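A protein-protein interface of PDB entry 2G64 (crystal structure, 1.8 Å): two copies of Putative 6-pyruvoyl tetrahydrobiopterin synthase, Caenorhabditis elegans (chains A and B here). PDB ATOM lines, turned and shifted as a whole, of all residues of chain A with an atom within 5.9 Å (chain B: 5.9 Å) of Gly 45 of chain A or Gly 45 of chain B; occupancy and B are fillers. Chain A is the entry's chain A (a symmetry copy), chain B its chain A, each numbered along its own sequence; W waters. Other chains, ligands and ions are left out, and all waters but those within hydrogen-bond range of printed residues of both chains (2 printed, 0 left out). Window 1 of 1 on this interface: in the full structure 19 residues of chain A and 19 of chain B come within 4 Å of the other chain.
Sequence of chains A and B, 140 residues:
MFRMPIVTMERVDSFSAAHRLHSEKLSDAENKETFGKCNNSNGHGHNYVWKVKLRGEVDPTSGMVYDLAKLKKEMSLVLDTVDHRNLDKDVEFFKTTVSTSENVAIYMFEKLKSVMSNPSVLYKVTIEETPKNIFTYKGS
A ring nitrogen (ND1) of His 46 of chain A sits at hydrogen-bond distance from the side-chain amide oxygen of Asn 47 of chain B. A ring nitrogen (ND1) of His 46 of chain B lies within hydrogen-bond range of the side-chain amide oxygen of Asn 47 of chain A, at 2.8 Å. The backbone carbonyl oxygen of His 46 of chain B lies close to the backbone carbonyl oxygen of Gly 45 of chain A (3.3 Å). The backbone carbonyl oxygen of Gly 45 of chain B lies close to the backbone carbonyl oxygen of His 46 of chain A (3.3 Å). ND2 of Asn 47 of chain B is in hydrogen-bond range of O of Asn 47 of chain A (3.1 Å).
O of Arg 85 of chain A is in hydrogen-bond range of N of Ala 18 of chain A (2.9 Å). The side-chain hydroxyl of Ser 16 of chain A lies within hydrogen-bond range of the side-chain amide oxygen of Asn 47 of chain A (2.8 Å). OG of Ser 16 of chain B is in hydrogen-bond range of OD1 of Asn 47 of chain B, 2.8 Å away. The backbone carbonyl oxygen (O) of Arg 85 of chain B sits at hydrogen-bond distance from the backbone NH (N) of Ala 18 of chain B, at 2.9 Å. The backbone NH (N) of His 46 of chain B lies within hydrogen-bond range of the backbone carbonyl oxygen (O) of Ala 17 of chain B (3.0 Å). The backbone carbonyl oxygen of Ala 17 of chain A is in hydrogen-bond range of the backbone NH of His 46 of chain A, at 3.0 Å.
Among the printed residues, merely in contact across the chains: Ser 16 of chain A with Gly 45 of chain B (3.3 Å), Gly 45 of chain A with Ser 16 of chain B (3.3 Å), Gly 43 of chain A with Arg 85 of chain B (3.3 Å), Arg 85 of chain A with Gly 43 of chain B (3.3 Å), Ala 17 of chain A with Gly 45 of chain B (3.4 Å), Gly 45 of chain A with Ala 17 of chain B (3.4 Å), Ala 18 of chain A with His 44 of chain B (3.5 Å), His 44 of chain A with Ala 18 of chain B (3.5 Å), Ser 16 of chain A with His 46 of chain B (3.5 Å), His 46 of chain A with Ser 16 of chain B (3.5 Å), Ala 18 of chain A with Gly 45 of chain B (3.7 Å), Gly 45 of chain A with Ala 18 of chain B (3.7 Å), His 46 of chain A with His 46 of chain B (3.7 Å), Asn 47 of chain A with Gly 45 of chain B (3.7 Å), Gly 45 of chain A with Asn 47 of chain B (3.7 Å), Gly 45 of chain A with Gly 45 of chain B (3.8 Å), Ala 17 of chain A with His 44 of chain B (3.8 Å), His 44 of chain A with Arg 85 of chain B (3.8 Å), His 44 of chain A with Ala 17 of chain B (3.8 Å) and Arg 85 of chain A with His 44 of chain B (3.8 Å).
Phe 15 of chain A touches none of the printed residues of chain B. Of the printed residues of chain B, Ala 18 of chain A touches His 44 and Gly 45. Of the printed residues of chain B, His 44 of chain A touches Ala 17 (3.8 Å), Ala 18 (3.5 Å) and Arg 85 (3.8 Å). Of the printed residues of chain A, Ala 17 of chain B touches His 44 and Gly 45. His 19 of chain B touches none of the printed residues of chain A. Of the printed residues of chain A, Gly 45 of chain B touches Ser 16, Ala 17, Ala 18, Gly 45, His 46 and Asn 47. Printed residues of chain A within 4 Å of Asn 47 of chain B: Gly 45, His 46 and Asn 47.
Of the 12 printed residues of chain B, 9 touch a printed residue of chain A. Of the 12 printed residues of chain A, 9 touch a printed residue of chain B. Hydrophobic or aromatic side chains of chain A that line the printed part of chain B: Ala 18 and His 46. Among the printed residues, 25 pairs touch across the chains.
Ala 17 of chain A touches His 44 of chain B, and with the chains exchanged His 44 of chain A touches Ala 17 of chain B. Ala 18 of chain A touches Gly 45 of chain B, and with the chains exchanged Gly 45 of chain A touches Ala 18 of chain B. Gly 45 of chain A touches His 46 of chain B, and with the chains exchanged His 46 of chain A touches Gly 45 of chain B. His 46 of chain A touches Asn 47 of chain B, and with the chains exchanged Asn 47 of chain A touches His 46 of chain B. 12 positions are printed for both chains. Of the 25 pairs that touch across the chains among the printed residues, 25 have their exchanged pair printed and touching as well.
Water W2 lies within hydrogen-bond range of the side-chain amide nitrogen of Asn 47 of chain B (2.6 Å) and the backbone carbonyl oxygen of Asn 47 of chain A (3.3 Å). Water W1 bridges ND2 of Asn 47 of chain A and O of Asn 47 of chain B.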
ATOM      1  N   PHE A  15      15.941  22.662   1.910  1.00  0.00           N
ATOM      2  CA  PHE A  15      14.928  21.607   2.057  1.00  0.00           C
ATOM      3  C   PHE A  15      14.472  21.108   0.685  1.00  0.00           C
ATOM      4  O   PHE A  15      14.495  21.841  -0.295  1.00  0.00           O
ATOM      5  CB  PHE A  15      13.743  22.057   2.934  1.00  0.00           C
ATOM      6  CG  PHE A  15      12.947  23.240   2.378  1.00  0.00           C
ATOM      7  CD1 PHE A  15      11.779  23.031   1.650  1.00  0.00           C
ATOM      8  CD2 PHE A  15      13.353  24.561   2.631  1.00  0.00           C
ATOM      9  CE1 PHE A  15      11.039  24.112   1.145  1.00  0.00           C
ATOM     10  CE2 PHE A  15      12.632  25.655   2.135  1.00  0.00           C
ATOM     11  CZ  PHE A  15      11.461  25.433   1.391  1.00  0.00           C
ATOM     12  N   SER A  16      14.087  19.844   0.617  1.00  0.00           N
ATOM     13  CA  SER A  16      13.633  19.283  -0.642  1.00  0.00           C
ATOM     14  C   SER A  16      12.118  19.114  -0.570  1.00  0.00           C
ATOM     15  O   SER A  16      11.581  18.624   0.424  1.00  0.00           O
ATOM     16  CB  SER A  16      14.363  17.967  -0.924  1.00  0.00           C
ATOM     17  OG  SER A  16      15.752  18.196  -1.125  1.00  0.00           O
ATOM     18  N   ALA A  17      11.413  19.588  -1.594  1.00  0.00           N
ATOM     19  CA  ALA A  17       9.959  19.488  -1.541  1.00  0.00           C
ATOM     20  C   ALA A  17       9.373  19.377  -2.935  1.00  0.00           C
ATOM     21  O   ALA A  17       9.961  19.849  -3.923  1.00  0.00           O
ATOM     22  CB  ALA A  17       9.341  20.691  -0.792  1.00  0.00           C
ATOM     23  N   ALA A  18       8.198  18.760  -3.004  1.00  0.00           N
ATOM     24  CA  ALA A  18       7.407  18.751  -4.221  1.00  0.00           C
ATOM     25  C   ALA A  18       6.370  19.873  -4.164  1.00  0.00           C
ATOM     26  O   ALA A  18       5.910  20.263  -3.086  1.00  0.00           O
ATOM     27  CB  ALA A  18       6.689  17.375  -4.367  1.00  0.00           C
ATOM     28  N   HIS A  19       5.963  20.352  -5.325  1.00  0.00           N
ATOM     29  CA  HIS A  19       4.784  21.214  -5.397  1.00  0.00           C
ATOM     30  C   HIS A  19       4.184  21.230  -6.794  1.00  0.00           C
ATOM     31  O   HIS A  19       4.758  20.671  -7.741  1.00  0.00           O
ATOM     32  CB  HIS A  19       5.110  22.635  -4.864  1.00  0.00           C
ATOM     33  CG  HIS A  19       5.809  23.533  -5.844  1.00  0.00           C
ATOM     34  ND1 HIS A  19       5.553  24.889  -5.909  1.00  0.00           N
ATOM     35  CD2 HIS A  19       6.786  23.293  -6.756  1.00  0.00           C
ATOM     36  CE1 HIS A  19       6.315  25.444  -6.837  1.00  0.00           C
ATOM     37  NE2 HIS A  19       7.086  24.498  -7.355  1.00  0.00           N
ATOM     38  N   GLY A  43       2.833  17.329 -10.441  1.00  0.00           N
ATOM     39  CA  GLY A  43       3.775  18.158  -9.713  1.00  0.00           C
ATOM     40  C   GLY A  43       5.210  18.028 -10.222  1.00  0.00           C
ATOM     41  O   GLY A  43       5.502  17.370 -11.250  1.00  0.00           O
ATOM     42  N   HIS A  44       6.099  18.703  -9.509  1.00  0.00           N
ATOM     43  CA  HIS A  44       7.527  18.680  -9.787  1.00  0.00           C
ATOM     44  C   HIS A  44       8.120  19.111  -8.448  1.00  0.00           C
ATOM     45  O   HIS A  44       7.417  19.072  -7.421  1.00  0.00           O
ATOM     46  CB  HIS A  44       7.904  19.643 -10.937  1.00  0.00           C
ATOM     47  CG  HIS A  44       7.601  21.092 -10.659  1.00  0.00           C
ATOM     48  ND1 HIS A  44       6.321  21.610 -10.698  1.00  0.00           N
ATOM     49  CD2 HIS A  44       8.412  22.127 -10.316  1.00  0.00           C
ATOM     50  CE1 HIS A  44       6.356  22.897 -10.391  1.00  0.00           C
ATOM     51  NE2 HIS A  44       7.612  23.235 -10.155  1.00  0.00           N
ATOM     52  N   GLY A  45       9.394  19.487  -8.430  1.00  0.00           N
ATOM     53  CA  GLY A  45      10.040  19.720  -7.143  1.00  0.00           C
ATOM     54  C   GLY A  45      11.322  20.513  -7.218  1.00  0.00           C
ATOM     55  O   GLY A  45      11.808  20.817  -8.303  1.00  0.00           O
ATOM     56  N   HIS A  46      11.855  20.862  -6.051  1.00  0.00           N
ATOM     57  CA  HIS A  46      13.047  21.710  -5.987  1.00  0.00           C
ATOM     58  C   HIS A  46      13.825  21.338  -4.747  1.00  0.00           C
ATOM     59  O   HIS A  46      13.238  20.895  -3.755  1.00  0.00           O
ATOM     60  CB  HIS A  46      12.690  23.214  -5.912  1.00  0.00           C
ATOM     61  CG  HIS A  46      11.900  23.715  -7.079  1.00  0.00           C
ATOM     62  ND1 HIS A  46      12.440  23.849  -8.337  1.00  0.00           N
ATOM     63  CD2 HIS A  46      10.601  24.088  -7.184  1.00  0.00           C
ATOM     64  CE1 HIS A  46      11.510  24.290  -9.169  1.00  0.00           C
ATOM     65  NE2 HIS A  46      10.387  24.444  -8.493  1.00  0.00           N
ATOM     66  N   ASN A  47      15.149  21.524  -4.787  1.00  0.00           N
ATOM     67  CA  ASN A  47      15.899  21.756  -3.551  1.00  0.00           C
ATOM     68  C   ASN A  47      15.865  23.252  -3.300  1.00  0.00           C
ATOM     69  O   ASN A  47      16.410  24.019  -4.081  1.00  0.00           O
ATOM     70  CB  ASN A  47      17.350  21.320  -3.718  1.00  0.00           C
ATOM     71  CG  ASN A  47      17.467  19.891  -4.186  1.00  0.00           C
ATOM     72  OD1 ASN A  47      16.881  18.979  -3.599  1.00  0.00           O
ATOM     73  ND2 ASN A  47      18.245  19.689  -5.243  1.00  0.00           N
ATOM     74  N   TYR A  48      15.163  23.666  -2.252  1.00  0.00           N
ATOM     75  CA  TYR A  48      15.031  25.085  -1.990  1.00  0.00           C
ATOM     76  C   TYR A  48      16.186  25.471  -1.062  1.00  0.00           C
ATOM     77  O   TYR A  48      16.404  24.812  -0.052  1.00  0.00           O
ATOM     78  CB  TYR A  48      13.705  25.341  -1.270  1.00  0.00           C
ATOM     79  CG  TYR A  48      12.460  25.223  -2.112  1.00  0.00           C
ATOM     80  CD1 TYR A  48      11.955  26.329  -2.798  1.00  0.00           C
ATOM     81  CD2 TYR A  48      11.744  24.016  -2.175  1.00  0.00           C
ATOM     82  CE1 TYR A  48      10.774  26.244  -3.560  1.00  0.00           C
ATOM     83  CE2 TYR A  48      10.563  23.926  -2.914  1.00  0.00           C
ATOM     84  CZ  TYR A  48      10.094  25.029  -3.612  1.00  0.00           C
ATOM     85  OH  TYR A  48       8.941  24.918  -4.331  1.00  0.00           O
ATOM     86  N   ARG A  85       8.589  17.008   1.968  1.00  0.00           N
ATOM     87  CA  ARG A  85       7.144  17.071   1.913  1.00  0.00           C
ATOM     88  C   ARG A  85       6.649  17.590   0.564  1.00  0.00           C
ATOM     89  O   ARG A  85       7.421  18.085  -0.268  1.00  0.00           O
ATOM     90  CB  ARG A  85       6.618  17.980   3.032  1.00  0.00           C
ATOM     91  CG  ARG A  85       7.099  17.552   4.431  1.00  0.00           C
ATOM     92  CD  ARG A  85       5.979  17.711   5.440  1.00  0.00           C
ATOM     93  NE  ARG A  85       6.460  17.683   6.816  1.00  0.00           N
ATOM     94  CZ  ARG A  85       6.385  16.621   7.612  1.00  0.00           C
ATOM     95  NH1 ARG A  85       5.851  15.490   7.169  1.00  0.00           N
ATOM     96  NH2 ARG A  85       6.846  16.689   8.855  1.00  0.00           N
ATOM     97  N   PHE B  15      17.291  19.671 -14.298  1.00  0.00           N
ATOM     98  CA  PHE B  15      15.836  19.505 -14.424  1.00  0.00           C
ATOM     99  C   PHE B  15      15.180  19.454 -13.044  1.00  0.00           C
ATOM    100  O   PHE B  15      15.790  19.034 -12.070  1.00  0.00           O
ATOM    101  CB  PHE B  15      15.464  18.285 -15.290  1.00  0.00           C
ATOM    102  CG  PHE B  15      15.929  16.938 -14.731  1.00  0.00           C
ATOM    103  CD1 PHE B  15      15.063  16.140 -13.987  1.00  0.00           C
ATOM    104  CD2 PHE B  15      17.221  16.457 -14.998  1.00  0.00           C
ATOM    105  CE1 PHE B  15      15.480  14.900 -13.479  1.00  0.00           C
ATOM    106  CE2 PHE B  15      17.660  15.223 -14.499  1.00  0.00           C
ATOM    107  CZ  PHE B  15      16.782  14.432 -13.739  1.00  0.00           C
ATOM    108  N   SER B  16      13.943  19.915 -12.963  1.00  0.00           N
ATOM    109  CA  SER B  16      13.239  19.903 -11.695  1.00  0.00           C
ATOM    110  C   SER B  16      12.184  18.801 -11.747  1.00  0.00           C
ATOM    111  O   SER B  16      11.455  18.665 -12.730  1.00  0.00           O
ATOM    112  CB  SER B  16      12.638  21.283 -11.414  1.00  0.00           C
ATOM    113  OG  SER B  16      13.666  22.249 -11.232  1.00  0.00           O
ATOM    114  N   ALA B  17      12.146  17.959 -10.716  1.00  0.00           N
ATOM    115  CA  ALA B  17      11.184  16.864 -10.750  1.00  0.00           C
ATOM    116  C   ALA B  17      10.758  16.474  -9.348  1.00  0.00           C
ATOM    117  O   ALA B  17      11.503  16.662  -8.371  1.00  0.00           O
ATOM    118  CB  ALA B  17      11.755  15.639 -11.498  1.00  0.00           C
ATOM    119  N   ALA B  18       9.555  15.915  -9.260  1.00  0.00           N
ATOM    120  CA  ALA B  18       9.084  15.300  -8.034  1.00  0.00           C
ATOM    121  C   ALA B  18       9.345  13.794  -8.084  1.00  0.00           C
ATOM    122  O   ALA B  18       9.363  13.185  -9.159  1.00  0.00           O
ATOM    123  CB  ALA B  18       7.557  15.564  -7.869  1.00  0.00           C
ATOM    124  N   HIS B  19       9.494  13.187  -6.921  1.00  0.00           N
ATOM    125  CA  HIS B  19       9.465  11.728  -6.839  1.00  0.00           C
ATOM    126  C   HIS B  19       9.132  11.251  -5.435  1.00  0.00           C
ATOM    127  O   HIS B  19       9.048  12.052  -4.491  1.00  0.00           O
ATOM    128  CB  HIS B  19      10.786  11.121  -7.386  1.00  0.00           C
ATOM    129  CG  HIS B  19      11.936  11.138  -6.420  1.00  0.00           C
ATOM    130  ND1 HIS B  19      12.860  10.112  -6.361  1.00  0.00           N
ATOM    131  CD2 HIS B  19      12.350  12.066  -5.519  1.00  0.00           C
ATOM    132  CE1 HIS B  19      13.774  10.387  -5.445  1.00  0.00           C
ATOM    133  NE2 HIS B  19      13.498  11.577  -4.932  1.00  0.00           N
ATOM    134  N   GLY B  43       5.258  12.567  -1.746  1.00  0.00           N
ATOM    135  CA  GLY B  43       6.480  12.808  -2.491  1.00  0.00           C
ATOM    136  C   GLY B  43       7.253  14.030  -2.000  1.00  0.00           C
ATOM    137  O   GLY B  43       6.920  14.668  -0.971  1.00  0.00           O
ATOM    138  N   HIS B  44       8.320  14.323  -2.728  1.00  0.00           N
ATOM    139  CA  HIS B  44       9.172  15.474  -2.469  1.00  0.00           C
ATOM    140  C   HIS B  44       9.857  15.675  -3.818  1.00  0.00           C
ATOM    141  O   HIS B  44       9.386  15.133  -4.836  1.00  0.00           O
ATOM    142  CB  HIS B  44      10.180  15.197  -1.330  1.00  0.00           C
ATOM    143  CG  HIS B  44      11.145  14.074  -1.613  1.00  0.00           C
ATOM    144  ND1 HIS B  44      10.780  12.743  -1.561  1.00  0.00           N
ATOM    145  CD2 HIS B  44      12.455  14.089  -1.973  1.00  0.00           C
ATOM    146  CE1 HIS B  44      11.820  11.988  -1.877  1.00  0.00           C
ATOM    147  NE2 HIS B  44      12.848  12.779  -2.130  1.00  0.00           N
ATOM    148  N   GLY B  45      10.928  16.459  -3.854  1.00  0.00           N
ATOM    149  CA  GLY B  45      11.489  16.823  -5.151  1.00  0.00           C
ATOM    150  C   GLY B  45      12.897  17.361  -5.098  1.00  0.00           C
ATOM    151  O   GLY B  45      13.449  17.571  -4.021  1.00  0.00           O
ATOM    152  N   HIS B  46      13.484  17.566  -6.273  1.00  0.00           N
ATOM    153  CA  HIS B  46      14.880  17.998  -6.359  1.00  0.00           C
ATOM    154  C   HIS B  46      15.041  18.834  -7.606  1.00  0.00           C
ATOM    155  O   HIS B  46      14.320  18.631  -8.587  1.00  0.00           O
ATOM    156  CB  HIS B  46      15.858  16.802  -6.438  1.00  0.00           C
ATOM    157  CG  HIS B  46      15.792  15.877  -5.265  1.00  0.00           C
ATOM    158  ND1 HIS B  46      16.242  16.233  -4.014  1.00  0.00           N
ATOM    159  CD2 HIS B  46      15.301  14.619  -5.145  1.00  0.00           C
ATOM    160  CE1 HIS B  46      16.039  15.232  -3.173  1.00  0.00           C
ATOM    161  NE2 HIS B  46      15.472  14.241  -3.836  1.00  0.00           N
ATOM    162  N   ASN B  47      15.993  19.774  -7.584  1.00  0.00           N
ATOM    163  CA  ASN B  47      16.616  20.223  -8.831  1.00  0.00           C
ATOM    164  C   ASN B  47      17.781  19.286  -9.091  1.00  0.00           C
ATOM    165  O   ASN B  47      18.731  19.258  -8.322  1.00  0.00           O
ATOM    166  CB  ASN B  47      17.152  21.641  -8.680  1.00  0.00           C
ATOM    167  CG  ASN B  47      16.093  22.604  -8.204  1.00  0.00           C
ATOM    168  OD1 ASN B  47      15.005  22.688  -8.777  1.00  0.00           O
ATOM    169  ND2 ASN B  47      16.418  23.352  -7.156  1.00  0.00           N
ATOM    170  N   TYR B  48      17.671  18.470 -10.133  1.00  0.00           N
ATOM    171  CA  TYR B  48      18.715  17.503 -10.402  1.00  0.00           C
ATOM    172  C   TYR B  48      19.711  18.180 -11.347  1.00  0.00           C
ATOM    173  O   TYR B  48      19.306  18.746 -12.356  1.00  0.00           O
ATOM    174  CB  TYR B  48      18.105  16.288 -11.106  1.00  0.00           C
ATOM    175  CG  TYR B  48      17.266  15.375 -10.248  1.00  0.00           C
ATOM    176  CD1 TYR B  48      17.848  14.307  -9.562  1.00  0.00           C
ATOM    177  CD2 TYR B  48      15.874  15.539 -10.168  1.00  0.00           C
ATOM    178  CE1 TYR B  48      17.073  13.425  -8.785  1.00  0.00           C
ATOM    179  CE2 TYR B  48      15.095  14.660  -9.413  1.00  0.00           C
ATOM    180  CZ  TYR B  48      15.696  13.622  -8.716  1.00  0.00           C
ATOM    181  OH  TYR B  48      14.918  12.777  -7.981  1.00  0.00           O
ATOM    182  N   ARG B  85       8.336  17.257 -14.225  1.00  0.00           N
ATOM    183  CA  ARG B  85       7.510  16.071 -14.152  1.00  0.00           C
ATOM    184  C   ARG B  85       7.640  15.372 -12.800  1.00  0.00           C
ATOM    185  O   ARG B  85       8.512  15.691 -11.982  1.00  0.00           O
ATOM    186  CB  ARG B  85       7.899  15.095 -15.270  1.00  0.00           C
ATOM    187  CG  ARG B  85       7.833  15.728 -16.673  1.00  0.00           C
ATOM    188  CD  ARG B  85       7.267  14.734 -17.668  1.00  0.00           C
ATOM    189  NE  ARG B  85       7.519  15.126 -19.050  1.00  0.00           N
ATOM    190  CZ  ARG B  85       6.619  15.705 -19.838  1.00  0.00           C
ATOM    191  NH1 ARG B  85       5.402  15.970 -19.381  1.00  0.00           N
ATOM    192  NH2 ARG B  85       6.937  16.022 -21.087  1.00  0.00           N
HETATM  193  O   HOH W   1      19.933  21.429  -6.135  1.00  0.00           O
HETATM  194  O   HOH W   2      18.836  23.643  -6.297  1.00  0.00           O
